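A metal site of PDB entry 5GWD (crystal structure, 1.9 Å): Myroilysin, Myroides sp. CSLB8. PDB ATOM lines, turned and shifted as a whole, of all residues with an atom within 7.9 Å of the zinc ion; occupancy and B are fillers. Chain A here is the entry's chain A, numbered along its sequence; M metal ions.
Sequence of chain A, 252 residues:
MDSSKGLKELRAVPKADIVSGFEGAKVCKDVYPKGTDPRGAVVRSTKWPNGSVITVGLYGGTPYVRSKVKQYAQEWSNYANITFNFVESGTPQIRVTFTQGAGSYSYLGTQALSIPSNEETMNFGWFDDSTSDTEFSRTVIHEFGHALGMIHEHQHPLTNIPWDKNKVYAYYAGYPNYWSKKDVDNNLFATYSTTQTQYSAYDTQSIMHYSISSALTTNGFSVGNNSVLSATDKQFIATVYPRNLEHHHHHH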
ATOM      1  N   VAL A  27       4.175 -33.596 -31.142  1.00  0.00           N
ATOM      2  CA  VAL A  27       2.937 -32.853 -31.323  1.00  0.00           C
ATOM      3  C   VAL A  27       2.474 -32.198 -30.034  1.00  0.00           C
ATOM      4  O   VAL A  27       2.237 -32.892 -29.041  1.00  0.00           O
ATOM      5  CB  VAL A  27       1.838 -33.767 -31.879  1.00  0.00           C
ATOM      6  CG1 VAL A  27       0.543 -32.982 -32.047  1.00  0.00           C
ATOM      7  CG2 VAL A  27       2.280 -34.336 -33.224  1.00  0.00           C
ATOM      8  N   CYS A  28       2.296 -30.884 -30.030  1.00  0.00           N
ATOM      9  CA  CYS A  28       1.557 -30.248 -28.951  1.00  0.00           C
ATOM     10  C   CYS A  28       0.080 -30.207 -29.343  1.00  0.00           C
ATOM     11  O   CYS A  28      -0.265 -29.672 -30.402  1.00  0.00           O
ATOM     12  CB  CYS A  28       2.080 -28.846 -28.643  1.00  0.00           C
ATOM     13  SG  CYS A  28       1.151 -28.113 -27.272  1.00  0.00           S
ATOM     14  N   LYS A  29      -0.778 -30.789 -28.509  1.00  0.00           N
ATOM     15  CA  LYS A  29      -2.210 -30.890 -28.766  1.00  0.00           C
ATOM     16  C   LYS A  29      -2.952 -29.798 -28.005  1.00  0.00           C
ATOM     17  O   LYS A  29      -2.762 -29.644 -26.795  1.00  0.00           O
ATOM     18  CB  LYS A  29      -2.733 -32.259 -28.347  1.00  0.00           C
ATOM     19  CG  LYS A  29      -2.164 -33.432 -29.111  1.00  0.00           C
ATOM     20  CD  LYS A  29      -2.638 -34.756 -28.498  1.00  0.00           C
ATOM     21  CE  LYS A  29      -2.304 -35.948 -29.386  1.00  0.00           C
ATOM     22  NZ  LYS A  29      -2.646 -37.239 -28.709  1.00  0.00           N
ATOM     23  N   ASP A  30      -3.812 -29.048 -28.703  1.00  0.00           N
ATOM     24  CA  ASP A  30      -4.758 -28.172 -27.997  1.00  0.00           C
ATOM     25  C   ASP A  30      -5.741 -29.050 -27.227  1.00  0.00           C
ATOM     26  O   ASP A  30      -6.244 -30.046 -27.752  1.00  0.00           O
ATOM     27  CB  ASP A  30      -5.530 -27.260 -28.973  1.00  0.00           C
ATOM     28  CG  ASP A  30      -4.610 -26.329 -29.790  1.00  0.00           C
ATOM     29  OD1 ASP A  30      -3.585 -25.865 -29.267  1.00  0.00           O
ATOM     30  OD2 ASP A  30      -4.955 -26.031 -30.961  1.00  0.00           O
ATOM     31  N   SER A 104       2.173 -33.927 -26.202  1.00  0.00           N
ATOM     32  CA  SER A 104       2.316 -33.032 -25.065  1.00  0.00           C
ATOM     33  C   SER A 104       1.191 -32.003 -25.113  1.00  0.00           C
ATOM     34  O   SER A 104       0.740 -31.590 -26.192  1.00  0.00           O
ATOM     35  CB  SER A 104       3.696 -32.373 -25.057  1.00  0.00           C
ATOM     36  OG  SER A 104       4.741 -33.361 -24.926  1.00  0.00           O
ATOM     37  N   TYR A 105       0.712 -31.609 -23.943  1.00  0.00           N
ATOM     38  CA  TYR A 105      -0.425 -30.695 -23.885  1.00  0.00           C
ATOM     39  C   TYR A 105      -0.560 -30.148 -22.471  1.00  0.00           C
ATOM     40  O   TYR A 105      -0.023 -30.710 -21.520  1.00  0.00           O
ATOM     41  CB  TYR A 105      -1.736 -31.365 -24.309  1.00  0.00           C
ATOM     42  CG  TYR A 105      -1.998 -32.695 -23.645  1.00  0.00           C
ATOM     43  CD1 TYR A 105      -2.626 -32.777 -22.404  1.00  0.00           C
ATOM     44  CD2 TYR A 105      -1.630 -33.874 -24.273  1.00  0.00           C
ATOM     45  CE1 TYR A 105      -2.834 -34.006 -21.803  1.00  0.00           C
ATOM     46  CE2 TYR A 105      -1.850 -35.081 -23.698  1.00  0.00           C
ATOM     47  CZ  TYR A 105      -2.451 -35.155 -22.473  1.00  0.00           C
ATOM     48  OH  TYR A 105      -2.636 -36.403 -21.936  1.00  0.00           O
ATOM     49  N   SER A 106      -1.288 -29.044 -22.366  1.00  0.00           N
ATOM     50  CA  SER A 106      -1.737 -28.545 -21.074  1.00  0.00           C
ATOM     51  C   SER A 106      -3.057 -27.830 -21.287  1.00  0.00           C
ATOM     52  O   SER A 106      -3.242 -27.179 -22.326  1.00  0.00           O
ATOM     53  CB  SER A 106      -0.723 -27.584 -20.447  1.00  0.00           C
ATOM     54  OG  SER A 106      -1.257 -27.038 -19.247  1.00  0.00           O
ATOM     55  N   LEU A 108      -5.471 -24.719 -20.516  1.00  0.00           N
ATOM     56  CA  LEU A 108      -5.073 -23.320 -20.545  1.00  0.00           C
ATOM     57  C   LEU A 108      -5.441 -22.622 -19.248  1.00  0.00           C
ATOM     58  O   LEU A 108      -6.638 -22.511 -18.913  1.00  0.00           O
ATOM     59  CB  LEU A 108      -5.761 -22.623 -21.718  1.00  0.00           C
ATOM     60  CG  LEU A 108      -5.326 -23.167 -23.081  1.00  0.00           C
ATOM     61  CD1 LEU A 108      -6.311 -22.757 -24.143  1.00  0.00           C
ATOM     62  CD2 LEU A 108      -3.953 -22.622 -23.427  1.00  0.00           C
ATOM     63  N   THR A 139      10.109 -27.401 -24.776  1.00  0.00           N
ATOM     64  CA  THR A 139       8.810 -28.018 -24.545  1.00  0.00           C
ATOM     65  C   THR A 139       8.275 -27.696 -23.157  1.00  0.00           C
ATOM     66  O   THR A 139       7.074 -27.445 -23.012  1.00  0.00           O
ATOM     67  CB  THR A 139       8.931 -29.529 -24.788  1.00  0.00           C
ATOM     68  OG1 THR A 139       9.193 -29.721 -26.184  1.00  0.00           O
ATOM     69  CG2 THR A 139       7.636 -30.245 -24.442  1.00  0.00           C
ATOM     70  N   HIS A 142       7.143 -23.973 -23.053  1.00  0.00           N
ATOM     71  CA  HIS A 142       5.956 -23.900 -23.893  1.00  0.00           C
ATOM     72  C   HIS A 142       4.715 -24.419 -23.175  1.00  0.00           C
ATOM     73  O   HIS A 142       3.664 -23.760 -23.183  1.00  0.00           O
ATOM     74  CB  HIS A 142       6.210 -24.716 -25.161  1.00  0.00           C
ATOM     75  CG  HIS A 142       5.060 -24.752 -26.120  1.00  0.00           C
ATOM     76  ND1 HIS A 142       4.942 -23.863 -27.162  1.00  0.00           N
ATOM     77  CD2 HIS A 142       3.997 -25.576 -26.210  1.00  0.00           C
ATOM     78  CE1 HIS A 142       3.845 -24.131 -27.839  1.00  0.00           C
ATOM     79  NE2 HIS A 142       3.256 -25.181 -27.293  1.00  0.00           N
ATOM     80  N   GLU A 143       4.793 -25.595 -22.559  1.00  0.00           N
ATOM     81  CA  GLU A 143       3.602 -26.171 -21.939  1.00  0.00           C
ATOM     82  C   GLU A 143       3.178 -25.402 -20.699  1.00  0.00           C
ATOM     83  O   GLU A 143       1.987 -25.257 -20.426  1.00  0.00           O
ATOM     84  CB  GLU A 143       3.799 -27.647 -21.600  1.00  0.00           C
ATOM     85  CG  GLU A 143       4.032 -28.581 -22.802  1.00  0.00           C
ATOM     86  CD  GLU A 143       2.917 -28.500 -23.868  1.00  0.00           C
ATOM     87  OE1 GLU A 143       1.788 -28.066 -23.567  1.00  0.00           O
ATOM     88  OE2 GLU A 143       3.172 -28.908 -25.016  1.00  0.00           O
ATOM     89  N   GLY A 145       3.700 -22.265 -20.441  1.00  0.00           N
ATOM     90  CA  GLY A 145       3.015 -21.142 -21.045  1.00  0.00           C
ATOM     91  C   GLY A 145       1.527 -21.364 -21.172  1.00  0.00           C
ATOM     92  O   GLY A 145       0.728 -20.514 -20.786  1.00  0.00           O
ATOM     93  N   HIS A 146       1.123 -22.505 -21.751  1.00  0.00           N
ATOM     94  CA  HIS A 146      -0.294 -22.868 -21.778  1.00  0.00           C
ATOM     95  C   HIS A 146      -0.888 -22.876 -20.381  1.00  0.00           C
ATOM     96  O   HIS A 146      -2.023 -22.409 -20.171  1.00  0.00           O
ATOM     97  CB  HIS A 146      -0.491 -24.248 -22.407  1.00  0.00           C
ATOM     98  CG  HIS A 146      -0.250 -24.301 -23.889  1.00  0.00           C
ATOM     99  ND1 HIS A 146      -0.775 -23.387 -24.765  1.00  0.00           N
ATOM    100  CD2 HIS A 146       0.467 -25.179 -24.635  1.00  0.00           C
ATOM    101  CE1 HIS A 146      -0.386 -23.683 -25.997  1.00  0.00           C
ATOM    102  NE2 HIS A 146       0.368 -24.772 -25.932  1.00  0.00           N
ATOM    103  N   MET A 150      -1.404 -18.936 -21.984  1.00  0.00           N
ATOM    104  CA  MET A 150      -0.965 -18.569 -23.331  1.00  0.00           C
ATOM    105  C   MET A 150      -1.485 -19.570 -24.362  1.00  0.00           C
ATOM    106  O   MET A 150      -1.453 -20.774 -24.148  1.00  0.00           O
ATOM    107  CB  MET A 150       0.564 -18.540 -23.424  1.00  0.00           C
ATOM    108  CG  MET A 150       1.253 -17.723 -22.362  1.00  0.00           C
ATOM    109  SD  MET A 150       0.993 -16.000 -22.702  1.00  0.00           S
ATOM    110  CE  MET A 150       2.085 -15.795 -24.123  1.00  0.00           C
ATOM    111  N   ILE A 151      -1.918 -19.062 -25.510  1.00  0.00           N
ATOM    112  CA  ILE A 151      -2.331 -19.899 -26.618  1.00  0.00           C
ATOM    113  C   ILE A 151      -1.183 -19.968 -27.626  1.00  0.00           C
ATOM    114  O   ILE A 151      -0.218 -19.240 -27.545  1.00  0.00           O
ATOM    115  CB  ILE A 151      -3.619 -19.378 -27.279  1.00  0.00           C
ATOM    116  CG1 ILE A 151      -3.372 -17.989 -27.887  1.00  0.00           C
ATOM    117  CG2 ILE A 151      -4.767 -19.316 -26.293  1.00  0.00           C
ATOM    118  CD1 ILE A 151      -4.608 -17.392 -28.590  1.00  0.00           C
ATOM    119  N   HIS A 152      -1.337 -20.841 -28.625  1.00  0.00           N
ATOM    120  CA  HIS A 152      -0.336 -20.960 -29.683  1.00  0.00           C
ATOM    121  C   HIS A 152      -0.203 -19.687 -30.520  1.00  0.00           C
ATOM    122  O   HIS A 152      -1.192 -19.012 -30.822  1.00  0.00           O
ATOM    123  CB  HIS A 152      -0.707 -22.116 -30.613  1.00  0.00           C
ATOM    124  CG  HIS A 152      -0.380 -23.448 -30.062  1.00  0.00           C
ATOM    125  ND1 HIS A 152      -1.183 -24.553 -30.247  1.00  0.00           N
ATOM    126  CD2 HIS A 152       0.678 -23.867 -29.313  1.00  0.00           C
ATOM    127  CE1 HIS A 152      -0.637 -25.593 -29.641  1.00  0.00           C
ATOM    128  NE2 HIS A 152       0.488 -25.196 -29.061  1.00  0.00           N
ATOM    129  N   GLU A 153       1.041 -19.394 -30.922  1.00  0.00           N
ATOM    130  CA  GLU A 153       1.358 -18.361 -31.902  1.00  0.00           C
ATOM    131  C   GLU A 153       1.579 -19.018 -33.259  1.00  0.00           C
ATOM    132  O   GLU A 153       2.426 -19.901 -33.398  1.00  0.00           O
ATOM    133  CB  GLU A 153       2.629 -17.598 -31.504  1.00  0.00           C
ATOM    134  CG  GLU A 153       2.469 -16.680 -30.308  1.00  0.00           C
ATOM    135  CD  GLU A 153       1.529 -15.510 -30.593  1.00  0.00           C
ATOM    136  OE1 GLU A 153       1.656 -14.894 -31.667  1.00  0.00           O
ATOM    137  OE2 GLU A 153       0.672 -15.205 -29.721  1.00  0.00           O
ATOM    138  N   TYR A 192      -5.656 -23.773 -37.979  1.00  0.00           N
ATOM    139  CA  TYR A 192      -4.324 -23.325 -38.352  1.00  0.00           C
ATOM    140  C   TYR A 192      -4.226 -22.912 -39.818  1.00  0.00           C
ATOM    141  O   TYR A 192      -3.136 -22.594 -40.294  1.00  0.00           O
ATOM    142  CB  TYR A 192      -3.302 -24.406 -37.976  1.00  0.00           C
ATOM    143  CG  TYR A 192      -3.276 -24.552 -36.468  1.00  0.00           C
ATOM    144  CD1 TYR A 192      -2.639 -23.605 -35.674  1.00  0.00           C
ATOM    145  CD2 TYR A 192      -3.971 -25.580 -35.820  1.00  0.00           C
ATOM    146  CE1 TYR A 192      -2.642 -23.695 -34.280  1.00  0.00           C
ATOM    147  CE2 TYR A 192      -3.968 -25.683 -34.435  1.00  0.00           C
ATOM    148  CZ  TYR A 192      -3.304 -24.735 -33.679  1.00  0.00           C
ATOM    149  OH  TYR A 192      -3.321 -24.809 -32.294  1.00  0.00           O
ATOM    150  N   ILE A 207       8.166 -18.355 -27.728  1.00  0.00           N
ATOM    151  CA  ILE A 207       8.191 -19.721 -27.227  1.00  0.00           C
ATOM    152  C   ILE A 207       6.865 -20.423 -27.515  1.00  0.00           C
ATOM    153  O   ILE A 207       6.823 -21.651 -27.619  1.00  0.00           O
ATOM    154  CB  ILE A 207       8.529 -19.708 -25.709  1.00  0.00           C
ATOM    155  CG1 ILE A 207       8.854 -21.117 -25.199  1.00  0.00           C
ATOM    156  CG2 ILE A 207       7.382 -19.137 -24.875  1.00  0.00           C
ATOM    157  CD1 ILE A 207      10.190 -21.612 -25.685  1.00  0.00           C
ATOM    158  N   MET A 208       5.782 -19.655 -27.699  1.00  0.00           N
ATOM    159  CA  MET A 208       4.478 -20.252 -27.931  1.00  0.00           C
ATOM    160  C   MET A 208       4.235 -20.608 -29.393  1.00  0.00           C
ATOM    161  O   MET A 208       3.124 -21.017 -29.753  1.00  0.00           O
ATOM    162  CB  MET A 208       3.383 -19.319 -27.431  1.00  0.00           C
ATOM    163  CG  MET A 208       3.420 -19.064 -25.924  1.00  0.00           C
ATOM    164  SD  MET A 208       3.666 -20.551 -24.913  1.00  0.00           S
ATOM    165  CE  MET A 208       2.328 -21.600 -25.490  1.00  0.00           C
ATOM    166  N   HIS A 209       5.263 -20.496 -30.232  1.00  0.00           N
ATOM    167  CA  HIS A 209       5.157 -20.873 -31.637  1.00  0.00           C
ATOM    168  C   HIS A 209       4.612 -22.287 -31.777  1.00  0.00           C
ATOM    169  O   HIS A 209       5.006 -23.194 -31.040  1.00  0.00           O
ATOM    170  CB  HIS A 209       6.534 -20.755 -32.298  1.00  0.00           C
ATOM    171  CG  HIS A 209       6.651 -21.495 -33.585  1.00  0.00           C
ATOM    172  ND1 HIS A 209       6.205 -20.984 -34.785  1.00  0.00           N
ATOM    173  CD2 HIS A 209       7.188 -22.707 -33.872  1.00  0.00           C
ATOM    174  CE1 HIS A 209       6.445 -21.850 -35.746  1.00  0.00           C
ATOM    175  NE2 HIS A 209       7.050 -22.901 -35.224  1.00  0.00           N
ATOM    176  N   TYR A 210       3.661 -22.480 -32.694  1.00  0.00           N
ATOM    177  CA  TYR A 210       3.089 -23.797 -32.950  1.00  0.00           C
ATOM    178  C   TYR A 210       3.922 -24.469 -34.039  1.00  0.00           C
ATOM    179  O   TYR A 210       3.948 -24.014 -35.192  1.00  0.00           O
ATOM    180  CB  TYR A 210       1.627 -23.678 -33.367  1.00  0.00           C
ATOM    181  CG  TYR A 210       0.938 -24.986 -33.663  1.00  0.00           C
ATOM    182  CD1 TYR A 210       0.748 -25.943 -32.679  1.00  0.00           C
ATOM    183  CD2 TYR A 210       0.468 -25.270 -34.935  1.00  0.00           C
ATOM    184  CE1 TYR A 210       0.108 -27.156 -32.952  1.00  0.00           C
ATOM    185  CE2 TYR A 210      -0.178 -26.467 -35.222  1.00  0.00           C
ATOM    186  CZ  TYR A 210      -0.362 -27.398 -34.227  1.00  0.00           C
ATOM    187  OH  TYR A 210      -1.009 -28.585 -34.518  1.00  0.00           O
ATOM    188  N   SER A 211       4.624 -25.544 -33.684  1.00  0.00           N
ATOM    189  CA  SER A 211       5.388 -26.297 -34.675  1.00  0.00           C
ATOM    190  C   SER A 211       4.592 -27.517 -35.091  1.00  0.00           C
ATOM    191  O   SER A 211       4.009 -28.208 -34.246  1.00  0.00           O
ATOM    192  CB  SER A 211       6.767 -26.682 -34.142  1.00  0.00           C
ATOM    193  OG  SER A 211       6.709 -27.091 -32.803  1.00  0.00           O
HETATM  194 ZN    ZN M   1       1.343 -25.898 -27.393  1.00  0.00          ZN
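SG of Cys 28 lies close to O of Ser 104 (3.7 Å).
O of Met 150 is in hydrogen-bond range of ND1 of His 146, at 2.8 Å.
ND1 of His 152 is in hydrogen-bond range of OH of Tyr 192, at 3.0 Å.
O of Ile 207 sits at hydrogen-bond distance from ND1 of His 142 (2.9 Å).
OE2 of Glu 143 sits close to SG of Cys 28.
A ring nitrogen (ND1) of His 152 sits at hydrogen-bond distance from the side-chain carboxylate (OD1) of Asp 30, at 2.9 Å.
The zinc ion is bound by NE2 of His 152 (2.0 Å), NE2 of His 142 (2.0 Å), NE2 of His 146 (2.1 Å) and SG of Cys 28 (2.2 Å).
Of the 23 residues printed, 4 come within 4 Å of the zinc ion.
The nearest printed residue that does not touch the zinc ion is Glu 143 (4.2 Å).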
